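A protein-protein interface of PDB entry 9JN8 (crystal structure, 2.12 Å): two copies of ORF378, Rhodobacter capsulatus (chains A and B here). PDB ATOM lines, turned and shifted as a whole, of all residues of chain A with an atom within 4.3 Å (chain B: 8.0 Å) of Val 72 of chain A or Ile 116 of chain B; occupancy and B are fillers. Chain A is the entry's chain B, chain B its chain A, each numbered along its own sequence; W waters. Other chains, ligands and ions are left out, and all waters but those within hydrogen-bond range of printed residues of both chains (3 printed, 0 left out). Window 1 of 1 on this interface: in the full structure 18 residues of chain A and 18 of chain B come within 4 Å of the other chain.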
ATOM      1  N   VAL A  61      17.093 -27.390  13.661  1.00  0.00           N
ATOM      2  CA  VAL A  61      16.291 -26.927  12.537  1.00  0.00           C
ATOM      3  C   VAL A  61      14.914 -27.555  12.666  1.00  0.00           C
ATOM      4  O   VAL A  61      14.718 -28.549  13.369  1.00  0.00           O
ATOM      5  CB  VAL A  61      16.898 -27.289  11.155  1.00  0.00           C
ATOM      6  CG1 VAL A  61      18.304 -26.744  11.017  1.00  0.00           C
ATOM      7  CG2 VAL A  61      16.867 -28.799  10.940  1.00  0.00           C
ATOM      8  N   ALA A  62      13.955 -26.971  11.962  1.00  0.00           N
ATOM      9  CA  ALA A  62      12.601 -27.494  11.938  1.00  0.00           C
ATOM     10  C   ALA A  62      12.105 -27.530  10.503  1.00  0.00           C
ATOM     11  O   ALA A  62      12.455 -26.665   9.697  1.00  0.00           O
ATOM     12  CB  ALA A  62      11.651 -26.648  12.799  1.00  0.00           C
ATOM     13  N   SER A  70       5.022 -31.740  11.347  1.00  0.00           N
ATOM     14  CA  SER A  70       6.142 -30.875  11.678  1.00  0.00           C
ATOM     15  C   SER A  70       7.228 -31.703  12.350  1.00  0.00           C
ATOM     16  O   SER A  70       6.935 -32.653  13.081  1.00  0.00           O
ATOM     17  CB  SER A  70       5.698 -29.730  12.582  1.00  0.00           C
ATOM     18  OG  SER A  70       4.727 -28.931  11.933  1.00  0.00           O
ATOM     19  N   TYR A  71       8.483 -31.359  12.080  1.00  0.00           N
ATOM     20  CA  TYR A  71       9.618 -32.063  12.657  1.00  0.00           C
ATOM     21  C   TYR A  71      10.654 -31.071  13.153  1.00  0.00           C
ATOM     22  O   TYR A  71      10.842 -30.004  12.568  1.00  0.00           O
ATOM     23  CB  TYR A  71      10.304 -32.984  11.655  1.00  0.00           C
ATOM     24  CG  TYR A  71       9.522 -34.187  11.190  1.00  0.00           C
ATOM     25  CD1 TYR A  71       9.610 -35.401  11.864  1.00  0.00           C
ATOM     26  CD2 TYR A  71       8.747 -34.132  10.037  1.00  0.00           C
ATOM     27  CE1 TYR A  71       8.919 -36.515  11.426  1.00  0.00           C
ATOM     28  CE2 TYR A  71       8.052 -35.246   9.590  1.00  0.00           C
ATOM     29  CZ  TYR A  71       8.142 -36.433  10.290  1.00  0.00           C
ATOM     30  OH  TYR A  71       7.457 -37.545   9.854  1.00  0.00           O
ATOM     31  N   VAL A  72      11.342 -31.448  14.229  1.00  0.00           N
ATOM     32  CA  VAL A  72      12.491 -30.715  14.743  1.00  0.00           C
ATOM     33  C   VAL A  72      13.658 -31.688  14.827  1.00  0.00           C
ATOM     34  O   VAL A  72      13.514 -32.789  15.368  1.00  0.00           O
ATOM     35  CB  VAL A  72      12.198 -30.080  16.122  1.00  0.00           C
ATOM     36  CG1 VAL A  72      13.408 -29.301  16.618  1.00  0.00           C
ATOM     37  CG2 VAL A  72      10.972 -29.176  16.059  1.00  0.00           C
ATOM     38  N   TYR A  73      14.803 -31.292  14.278  1.00  0.00           N
ATOM     39  CA  TYR A  73      16.020 -32.089  14.318  1.00  0.00           C
ATOM     40  C   TYR A  73      17.097 -31.297  15.040  1.00  0.00           C
ATOM     41  O   TYR A  73      17.150 -30.068  14.934  1.00  0.00           O
ATOM     42  CB  TYR A  73      16.503 -32.458  12.906  1.00  0.00           C
ATOM     43  CG  TYR A  73      15.440 -33.096  12.050  1.00  0.00           C
ATOM     44  CD1 TYR A  73      15.235 -34.470  12.072  1.00  0.00           C
ATOM     45  CD2 TYR A  73      14.628 -32.324  11.230  1.00  0.00           C
ATOM     46  CE1 TYR A  73      14.256 -35.054  11.302  1.00  0.00           C
ATOM     47  CE2 TYR A  73      13.647 -32.903  10.451  1.00  0.00           C
ATOM     48  CZ  TYR A  73      13.466 -34.268  10.493  1.00  0.00           C
ATOM     49  OH  TYR A  73      12.488 -34.854   9.724  1.00  0.00           O
ATOM     50  N   CYS A 112      16.099 -36.733  15.253  1.00  0.00           N
ATOM     51  CA  CYS A 112      14.822 -36.050  15.392  1.00  0.00           C
ATOM     52  C   CYS A 112      14.506 -35.863  16.876  1.00  0.00           C
ATOM     53  O   CYS A 112      14.561 -36.818  17.652  1.00  0.00           O
ATOM     54  CB  CYS A 112      13.726 -36.859  14.701  1.00  0.00           C
ATOM     55  SG  CYS A 112      12.082 -36.125  14.780  1.00  0.00           S
ATOM     56  N   LEU A 113      14.206 -34.626  17.272  1.00  0.00           N
ATOM     57  CA  LEU A 113      13.875 -34.314  18.658  1.00  0.00           C
ATOM     58  C   LEU A 113      12.383 -34.343  18.939  1.00  0.00           C
ATOM     59  O   LEU A 113      11.994 -34.480  20.104  1.00  0.00           O
ATOM     60  CB  LEU A 113      14.395 -32.921  19.038  1.00  0.00           C
ATOM     61  CG  LEU A 113      15.869 -32.583  18.801  1.00  0.00           C
ATOM     62  CD1 LEU A 113      16.121 -31.151  19.225  1.00  0.00           C
ATOM     63  CD2 LEU A 113      16.778 -33.537  19.563  1.00  0.00           C
ATOM     64  N   ALA A 114      11.545 -34.189  17.914  1.00  0.00           N
ATOM     65  CA  ALA A 114      10.103 -34.098  18.095  1.00  0.00           C
ATOM     66  C   ALA A 114       9.432 -34.089  16.735  1.00  0.00           C
ATOM     67  O   ALA A 114      10.019 -33.651  15.741  1.00  0.00           O
ATOM     68  CB  ALA A 114       9.711 -32.834  18.875  1.00  0.00           C
ATOM     69  N   ILE A 116       5.216 -33.263  15.272  1.00  0.00           N
ATOM     70  CA  ILE A 116       3.875 -32.812  15.637  1.00  0.00           C
ATOM     71  C   ILE A 116       2.933 -33.183  14.501  1.00  0.00           C
ATOM     72  O   ILE A 116       3.289 -33.004  13.327  1.00  0.00           O
ATOM     73  CB  ILE A 116       3.850 -31.301  15.916  1.00  0.00           C
ATOM     74  CG1 ILE A 116       4.917 -30.933  16.943  1.00  0.00           C
ATOM     75  CG2 ILE A 116       2.483 -30.858  16.410  1.00  0.00           C
ATOM     76  CD1 ILE A 116       4.918 -29.477  17.294  1.00  0.00           C
ATOM     77  N   LEU B  52       5.387 -38.940  19.475  1.00  0.00           N
ATOM     78  CA  LEU B  52       5.807 -37.596  19.101  1.00  0.00           C
ATOM     79  C   LEU B  52       7.302 -37.525  18.799  1.00  0.00           C
ATOM     80  O   LEU B  52       7.879 -36.435  18.825  1.00  0.00           O
ATOM     81  CB  LEU B  52       5.436 -36.595  20.203  1.00  0.00           C
ATOM     82  CG  LEU B  52       3.943 -36.325  20.433  1.00  0.00           C
ATOM     83  CD1 LEU B  52       3.699 -35.487  21.702  1.00  0.00           C
ATOM     84  CD2 LEU B  52       3.313 -35.645  19.227  1.00  0.00           C
ATOM     85  N   SER B  53       7.927 -38.672  18.513  1.00  0.00           N
ATOM     86  CA  SER B  53       9.362 -38.782  18.216  1.00  0.00           C
ATOM     87  C   SER B  53      10.234 -38.087  19.257  1.00  0.00           C
ATOM     88  O   SER B  53      11.343 -37.636  18.960  1.00  0.00           O
ATOM     89  CB  SER B  53       9.690 -38.255  16.817  1.00  0.00           C
ATOM     90  OG  SER B  53      11.034 -38.567  16.500  1.00  0.00           O
ATOM     91  N   LEU B  63       1.576 -28.879  22.051  1.00  0.00           N
ATOM     92  CA  LEU B  63       0.550 -27.850  21.971  1.00  0.00           C
ATOM     93  C   LEU B  63       0.657 -27.158  20.622  1.00  0.00           C
ATOM     94  O   LEU B  63       1.752 -26.758  20.209  1.00  0.00           O
ATOM     95  CB  LEU B  63       0.688 -26.822  23.095  1.00  0.00           C
ATOM     96  CG  LEU B  63       0.214 -27.231  24.491  1.00  0.00           C
ATOM     97  CD1 LEU B  63       0.613 -26.163  25.494  1.00  0.00           C
ATOM     98  CD2 LEU B  63      -1.296 -27.463  24.525  1.00  0.00           C
ATOM     99  N   SER B  64      -0.473 -27.019  19.938  1.00  0.00           N
ATOM    100  CA  SER B  64      -0.480 -26.316  18.668  1.00  0.00           C
ATOM    101  C   SER B  64      -1.877 -25.779  18.406  1.00  0.00           C
ATOM    102  O   SER B  64      -2.855 -26.197  19.029  1.00  0.00           O
ATOM    103  CB  SER B  64      -0.013 -27.225  17.527  1.00  0.00           C
ATOM    104  OG  SER B  64      -0.708 -28.456  17.556  1.00  0.00           O
ATOM    105  N   LYS B  68      -0.718 -20.024  15.908  1.00  0.00           N
ATOM    106  CA  LYS B  68       0.062 -20.031  17.133  1.00  0.00           C
ATOM    107  C   LYS B  68       1.361 -20.796  16.914  1.00  0.00           C
ATOM    108  O   LYS B  68       1.486 -21.613  15.995  1.00  0.00           O
ATOM    109  CB  LYS B  68      -0.725 -20.662  18.291  1.00  0.00           C
ATOM    110  CG  LYS B  68      -2.029 -19.959  18.654  1.00  0.00           C
ATOM    111  CD  LYS B  68      -2.730 -20.692  19.802  1.00  0.00           C
ATOM    112  CE  LYS B  68      -3.994 -19.982  20.279  1.00  0.00           C
ATOM    113  NZ  LYS B  68      -3.693 -18.787  21.116  1.00  0.00           N
ATOM    114  N   TRP B  69       2.336 -20.503  17.771  1.00  0.00           N
ATOM    115  CA  TRP B  69       3.525 -21.333  17.862  1.00  0.00           C
ATOM    116  C   TRP B  69       3.146 -22.746  18.283  1.00  0.00           C
ATOM    117  O   TRP B  69       2.137 -22.968  18.958  1.00  0.00           O
ATOM    118  CB  TRP B  69       4.511 -20.743  18.871  1.00  0.00           C
ATOM    119  CG  TRP B  69       5.222 -19.515  18.398  1.00  0.00           C
ATOM    120  CD1 TRP B  69       4.700 -18.258  18.270  1.00  0.00           C
ATOM    121  CD2 TRP B  69       6.599 -19.421  18.005  1.00  0.00           C
ATOM    122  NE1 TRP B  69       5.667 -17.390  17.817  1.00  0.00           N
ATOM    123  CE2 TRP B  69       6.840 -18.079  17.646  1.00  0.00           C
ATOM    124  CE3 TRP B  69       7.649 -20.343  17.919  1.00  0.00           C
ATOM    125  CZ2 TRP B  69       8.088 -17.637  17.202  1.00  0.00           C
ATOM    126  CZ3 TRP B  69       8.889 -19.900  17.482  1.00  0.00           C
ATOM    127  CH2 TRP B  69       9.097 -18.560  17.129  1.00  0.00           C
ATOM    128  N   SER B  70       3.959 -23.710  17.877  1.00  0.00           N
ATOM    129  CA  SER B  70       3.815 -25.081  18.337  1.00  0.00           C
ATOM    130  C   SER B  70       4.871 -25.357  19.399  1.00  0.00           C
ATOM    131  O   SER B  70       5.972 -24.810  19.346  1.00  0.00           O
ATOM    132  CB  SER B  70       3.941 -26.066  17.176  1.00  0.00           C
ATOM    133  OG  SER B  70       2.915 -25.854  16.220  1.00  0.00           O
ATOM    134  N   TYR B  71       4.522 -26.185  20.384  1.00  0.00           N
ATOM    135  CA  TYR B  71       5.436 -26.525  21.462  1.00  0.00           C
ATOM    136  C   TYR B  71       5.420 -28.026  21.699  1.00  0.00           C
ATOM    137  O   TYR B  71       4.390 -28.686  21.543  1.00  0.00           O
ATOM    138  CB  TYR B  71       5.073 -25.813  22.770  1.00  0.00           C
ATOM    139  CG  TYR B  71       5.395 -24.340  22.805  1.00  0.00           C
ATOM    140  CD1 TYR B  71       4.462 -23.398  22.394  1.00  0.00           C
ATOM    141  CD2 TYR B  71       6.623 -23.887  23.273  1.00  0.00           C
ATOM    142  CE1 TYR B  71       4.748 -22.040  22.440  1.00  0.00           C
ATOM    143  CE2 TYR B  71       6.918 -22.533  23.323  1.00  0.00           C
ATOM    144  CZ  TYR B  71       5.977 -21.615  22.904  1.00  0.00           C
ATOM    145  OH  TYR B  71       6.269 -20.270  22.952  1.00  0.00           O
ATOM    146  N   VAL B  72       6.569 -28.561  22.096  1.00  0.00           N
ATOM    147  CA  VAL B  72       6.671 -29.938  22.558  1.00  0.00           C
ATOM    148  C   VAL B  72       7.315 -29.912  23.934  1.00  0.00           C
ATOM    149  O   VAL B  72       8.361 -29.282  24.120  1.00  0.00           O
ATOM    150  CB  VAL B  72       7.484 -30.824  21.593  1.00  0.00           C
ATOM    151  CG1 VAL B  72       7.465 -32.278  22.073  1.00  0.00           C
ATOM    152  CG2 VAL B  72       6.931 -30.730  20.179  1.00  0.00           C
ATOM    153  N   PHE B  91      -2.043 -21.310  27.011  1.00  0.00           N
ATOM    154  CA  PHE B  91      -1.658 -21.317  25.604  1.00  0.00           C
ATOM    155  C   PHE B  91      -2.796 -20.820  24.721  1.00  0.00           C
ATOM    156  O   PHE B  91      -2.569 -20.064  23.770  1.00  0.00           O
ATOM    157  CB  PHE B  91      -1.220 -22.729  25.199  1.00  0.00           C
ATOM    158  CG  PHE B  91      -0.843 -22.875  23.748  1.00  0.00           C
ATOM    159  CD1 PHE B  91       0.441 -22.583  23.313  1.00  0.00           C
ATOM    160  CD2 PHE B  91      -1.760 -23.340  22.826  1.00  0.00           C
ATOM    161  CE1 PHE B  91       0.790 -22.735  21.979  1.00  0.00           C
ATOM    162  CE2 PHE B  91      -1.417 -23.496  21.495  1.00  0.00           C
ATOM    163  CZ  PHE B  91      -0.142 -23.191  21.068  1.00  0.00           C
ATOM    164  N   LYS B  96      -0.717 -15.620  19.941  1.00  0.00           N
ATOM    165  CA  LYS B  96       0.129 -16.521  19.153  1.00  0.00           C
ATOM    166  C   LYS B  96       0.637 -17.708  19.965  1.00  0.00           C
ATOM    167  O   LYS B  96       1.618 -18.350  19.579  1.00  0.00           O
ATOM    168  CB  LYS B  96       1.313 -15.775  18.530  1.00  0.00           C
ATOM    169  CG  LYS B  96       0.921 -14.739  17.499  1.00  0.00           C
ATOM    170  CD  LYS B  96       2.123 -13.937  17.042  1.00  0.00           C
ATOM    171  CE  LYS B  96       1.766 -13.070  15.853  1.00  0.00           C
ATOM    172  NZ  LYS B  96       1.298 -13.898  14.702  1.00  0.00           N
ATOM    173  N   LEU B  98       2.108 -17.452  22.751  1.00  0.00           N
ATOM    174  CA  LEU B  98       3.288 -17.009  23.496  1.00  0.00           C
ATOM    175  C   LEU B  98       2.851 -16.568  24.894  1.00  0.00           C
ATOM    176  O   LEU B  98       2.423 -15.430  25.105  1.00  0.00           O
ATOM    177  CB  LEU B  98       4.010 -15.900  22.735  1.00  0.00           C
ATOM    178  CG  LEU B  98       4.687 -16.336  21.420  1.00  0.00           C
ATOM    179  CD1 LEU B  98       5.102 -15.149  20.556  1.00  0.00           C
ATOM    180  CD2 LEU B  98       5.890 -17.229  21.700  1.00  0.00           C
ATOM    181  N   CYS B 112      10.600 -27.797  28.102  1.00  0.00           N
ATOM    182  CA  CYS B 112      10.249 -27.640  26.699  1.00  0.00           C
ATOM    183  C   CYS B 112      11.359 -28.229  25.835  1.00  0.00           C
ATOM    184  O   CYS B 112      12.545 -27.967  26.064  1.00  0.00           O
ATOM    185  CB  CYS B 112      10.020 -26.168  26.360  1.00  0.00           C
ATOM    186  SG  CYS B 112       9.571 -25.887  24.627  1.00  0.00           S
ATOM    187  N   LEU B 113      10.972 -29.041  24.854  1.00  0.00           N
ATOM    188  CA  LEU B 113      11.924 -29.717  23.985  1.00  0.00           C
ATOM    189  C   LEU B 113      12.124 -29.004  22.661  1.00  0.00           C
ATOM    190  O   LEU B 113      13.194 -29.134  22.056  1.00  0.00           O
ATOM    191  CB  LEU B 113      11.464 -31.150  23.702  1.00  0.00           C
ATOM    192  CG  LEU B 113      11.005 -31.983  24.896  1.00  0.00           C
ATOM    193  CD1 LEU B 113      10.445 -33.320  24.429  1.00  0.00           C
ATOM    194  CD2 LEU B 113      12.150 -32.185  25.877  1.00  0.00           C
ATOM    195  N   ALA B 114      11.114 -28.271  22.197  1.00  0.00           N
ATOM    196  CA  ALA B 114      11.165 -27.597  20.906  1.00  0.00           C
ATOM    197  C   ALA B 114       9.971 -26.667  20.790  1.00  0.00           C
ATOM    198  O   ALA B 114       8.922 -26.904  21.392  1.00  0.00           O
ATOM    199  CB  ALA B 114      11.156 -28.601  19.745  1.00  0.00           C
ATOM    200  N   ARG B 115      10.144 -25.609  20.005  1.00  0.00           N
ATOM    201  CA  ARG B 115       9.041 -24.773  19.562  1.00  0.00           C
ATOM    202  C   ARG B 115       9.198 -24.513  18.071  1.00  0.00           C
ATOM    203  O   ARG B 115      10.309 -24.548  17.534  1.00  0.00           O
ATOM    204  CB  ARG B 115       8.970 -23.452  20.332  1.00  0.00           C
ATOM    205  CG  ARG B 115      10.172 -22.558  20.158  1.00  0.00           C
ATOM    206  CD  ARG B 115       9.914 -21.176  20.711  1.00  0.00           C
ATOM    207  NE  ARG B 115      10.928 -20.245  20.239  1.00  0.00           N
ATOM    208  CZ  ARG B 115      10.818 -18.925  20.276  1.00  0.00           C
ATOM    209  NH1 ARG B 115       9.749 -18.333  20.785  1.00  0.00           N
ATOM    210  NH2 ARG B 115      11.801 -18.182  19.778  1.00  0.00           N
ATOM    211  N   ILE B 116       8.073 -24.278  17.403  1.00  0.00           N
ATOM    212  CA  ILE B 116       8.049 -24.074  15.955  1.00  0.00           C
ATOM    213  C   ILE B 116       7.247 -22.816  15.644  1.00  0.00           C
ATOM    214  O   ILE B 116       6.151 -22.633  16.200  1.00  0.00           O
ATOM    215  CB  ILE B 116       7.455 -25.293  15.230  1.00  0.00           C
ATOM    216  CG1 ILE B 116       8.217 -26.563  15.604  1.00  0.00           C
ATOM    217  CG2 ILE B 116       7.473 -25.093  13.716  1.00  0.00           C
ATOM    218  CD1 ILE B 116       7.741 -27.781  14.852  1.00  0.00           C
ATOM    219  N   PRO B 117       7.747 -21.931  14.780  1.00  0.00           N
ATOM    220  CA  PRO B 117       6.998 -20.721  14.456  1.00  0.00           C
ATOM    221  C   PRO B 117       5.637 -21.072  13.864  1.00  0.00           C
ATOM    222  O   PRO B 117       5.456 -22.163  13.303  1.00  0.00           O
ATOM    223  CB  PRO B 117       7.890 -20.016  13.426  1.00  0.00           C
ATOM    224  CG  PRO B 117       9.261 -20.521  13.709  1.00  0.00           C
ATOM    225  CD  PRO B 117       9.086 -21.939  14.162  1.00  0.00           C
ATOM    226  N   PRO B 118       4.663 -20.174  13.992  1.00  0.00           N
ATOM    227  CA  PRO B 118       3.328 -20.473  13.450  1.00  0.00           C
ATOM    228  C   PRO B 118       3.352 -20.594  11.931  1.00  0.00           C
ATOM    229  O   PRO B 118       4.083 -19.881  11.239  1.00  0.00           O
ATOM    230  CB  PRO B 118       2.475 -19.284  13.917  1.00  0.00           C
ATOM    231  CG  PRO B 118       3.445 -18.232  14.361  1.00  0.00           C
ATOM    232  CD  PRO B 118       4.683 -18.946  14.797  1.00  0.00           C
ATOM    233  N   GLN B 119       2.540 -21.515  11.418  1.00  0.00           N
ATOM    234  CA  GLN B 119       2.491 -21.784   9.983  1.00  0.00           C
ATOM    235  C   GLN B 119       1.871 -20.625   9.211  1.00  0.00           C
ATOM    236  O   GLN B 119       0.670 -20.372   9.305  1.00  0.00           O
ATOM    237  CB  GLN B 119       1.712 -23.073   9.703  1.00  0.00           C
ATOM    238  CG  GLN B 119       2.385 -24.352  10.195  1.00  0.00           C
ATOM    239  CD  GLN B 119       2.072 -25.555   9.314  1.00  0.00           C
ATOM    240  OE1 GLN B 119       1.421 -25.425   8.277  1.00  0.00           O
ATOM    241  NE2 GLN B 119       2.540 -26.732   9.723  1.00  0.00           N
HETATM  242  O   HOH W   1      11.025 -39.564  13.691  1.00  0.00           O
HETATM  243  O   HOH W   2       4.184 -26.294  12.011  1.00  0.00           O
HETATM  244  O   HOH W   3       3.798 -28.819   9.335  1.00  0.00           O
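The backbone carbonyl oxygen (O) of Ser 53 of chain B sits close to the backbone carbonyl oxygen (O) of Leu 113 of chain A (3.4 Å).
The side-chain hydroxyl (OG) of Ser 53 of chain B lies within hydrogen-bond range of the side-chain sulfur (SG) of Cys 112 of chain A.
The backbone NH (N) of Ile 116 of chain B sits at hydrogen-bond distance from the backbone carbonyl oxygen (O) of Ser 70 of chain B, at 2.9 Å.
O of Ala 114 of chain A sits at hydrogen-bond distance from SG of Cys 112 of chain A (3.4 Å).
O of Val 72 of chain A sits at hydrogen-bond distance from N of Leu 113 of chain A (2.7 Å).
The backbone NH (N) of Leu 113 of chain B lies within hydrogen-bond range of the backbone carbonyl oxygen (O) of Val 72 of chain B, 2.7 Å away.
The backbone carbonyl oxygen of Val 72 of chain B lies close to the side-chain sulfur of Cys 112 of chain B (3.6 Å).
The side-chain sulfur of Cys 112 of chain B sits at hydrogen-bond distance from the backbone carbonyl oxygen of Ala 114 of chain B.
CD1 of Ile 116 of chain B touches CB of Ser 70 of chain A (3.6 Å).
OG of Ser 70 of chain A touches NE2 of Gln 119 of chain B (3.8 Å).
Val 72 of chain A touches Ala 114 of chain B.
Ile 116 of chain B touches Val 72 of chain A.
CA of Ala 114 of chain A touches O of Leu 52 of chain B, 3.3 Å away.
Ser 53 of chain B touches Ala 114 of chain A (O to N, 3.6 Å).
CB of Ala 114 of chain A touches CG2 of Val 72 of chain B (3.7 Å).
Ile 116 of chain A touches Ser 70 of chain B (CD1 to CB, 3.6 Å).
Ile 116 of chain A touches Val 72 of chain B (CD1 to CG2, 3.7 Å).
Of chain B, only Ala 114 (3.7 Å) and Ile 116 (3.7 Å) come within 4 Å of Val 72 of chain A.
Of chain A, only Ser 70 and Val 72 come within 4 Å of Ile 116 of chain B.
Of the printed residues of chain A, Ala 114 of chain B touches Val 72.
Of the printed residues of chain A, Ser 70 of chain B touches Ile 116 (3.6 Å).
Tyr 71 of chain B touches none of the printed residues of chain A.
The nearest residue of chain B that does not touch Val 72 of chain A is Arg 115 of chain B (4.9 Å).
The nearest residue of chain A that does not touch Ile 116 of chain B is Ile 116 of chain A (4.1 Å).
The nearest printed residue of chain A that does not touch Val 72 of chain B is Leu 113 of chain A (5.4 Å).
Of the 20 printed residues of chain B, 7 touch a printed residue of chain A.
Hydrophobic or aromatic side chains of chain B within 4 Å of the printed part of chain A: Val 72, Ala 114 and Ile 116.
Of the 10 printed residues of chain A, 6 touch a printed residue of chain B.
Along chain A the printed residues that touch a printed residue of chain B span positions 70 to 116.
Among the printed residues, 11 pairs touch across the chains.
Ser 70 of chain A touches Ile 116 of chain B, and with the chains exchanged Ile 116 of chain A touches Ser 70 of chain B.
Val 72 of chain A touches Ala 114 of chain B, and with the chains exchanged Ala 114 of chain A touches Val 72 of chain B.
Val 72 of chain A touches Ile 116 of chain B, and with the chains exchanged Ile 116 of chain A touches Val 72 of chain B.
7 positions are printed for both chains.
Of the 11 pairs that touch across the chains among the printed residues, 6 have their exchanged pair printed and touching as well.
Water W3 lies within hydrogen-bond range of the side-chain amide nitrogen of Gln 119 of chain B and the side-chain hydroxyl of Ser 70 of chain A.
Water W2 lies within hydrogen-bond range of OG of Ser 70 of chain A (2.7 Å) and NE2 of Gln 119 of chain B (2.9 Å).
Water W1 lies within hydrogen-bond range of OG of Ser 53 of chain B (3.0 Å) and SG of Cys 112 of chain A (3.8 Å).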
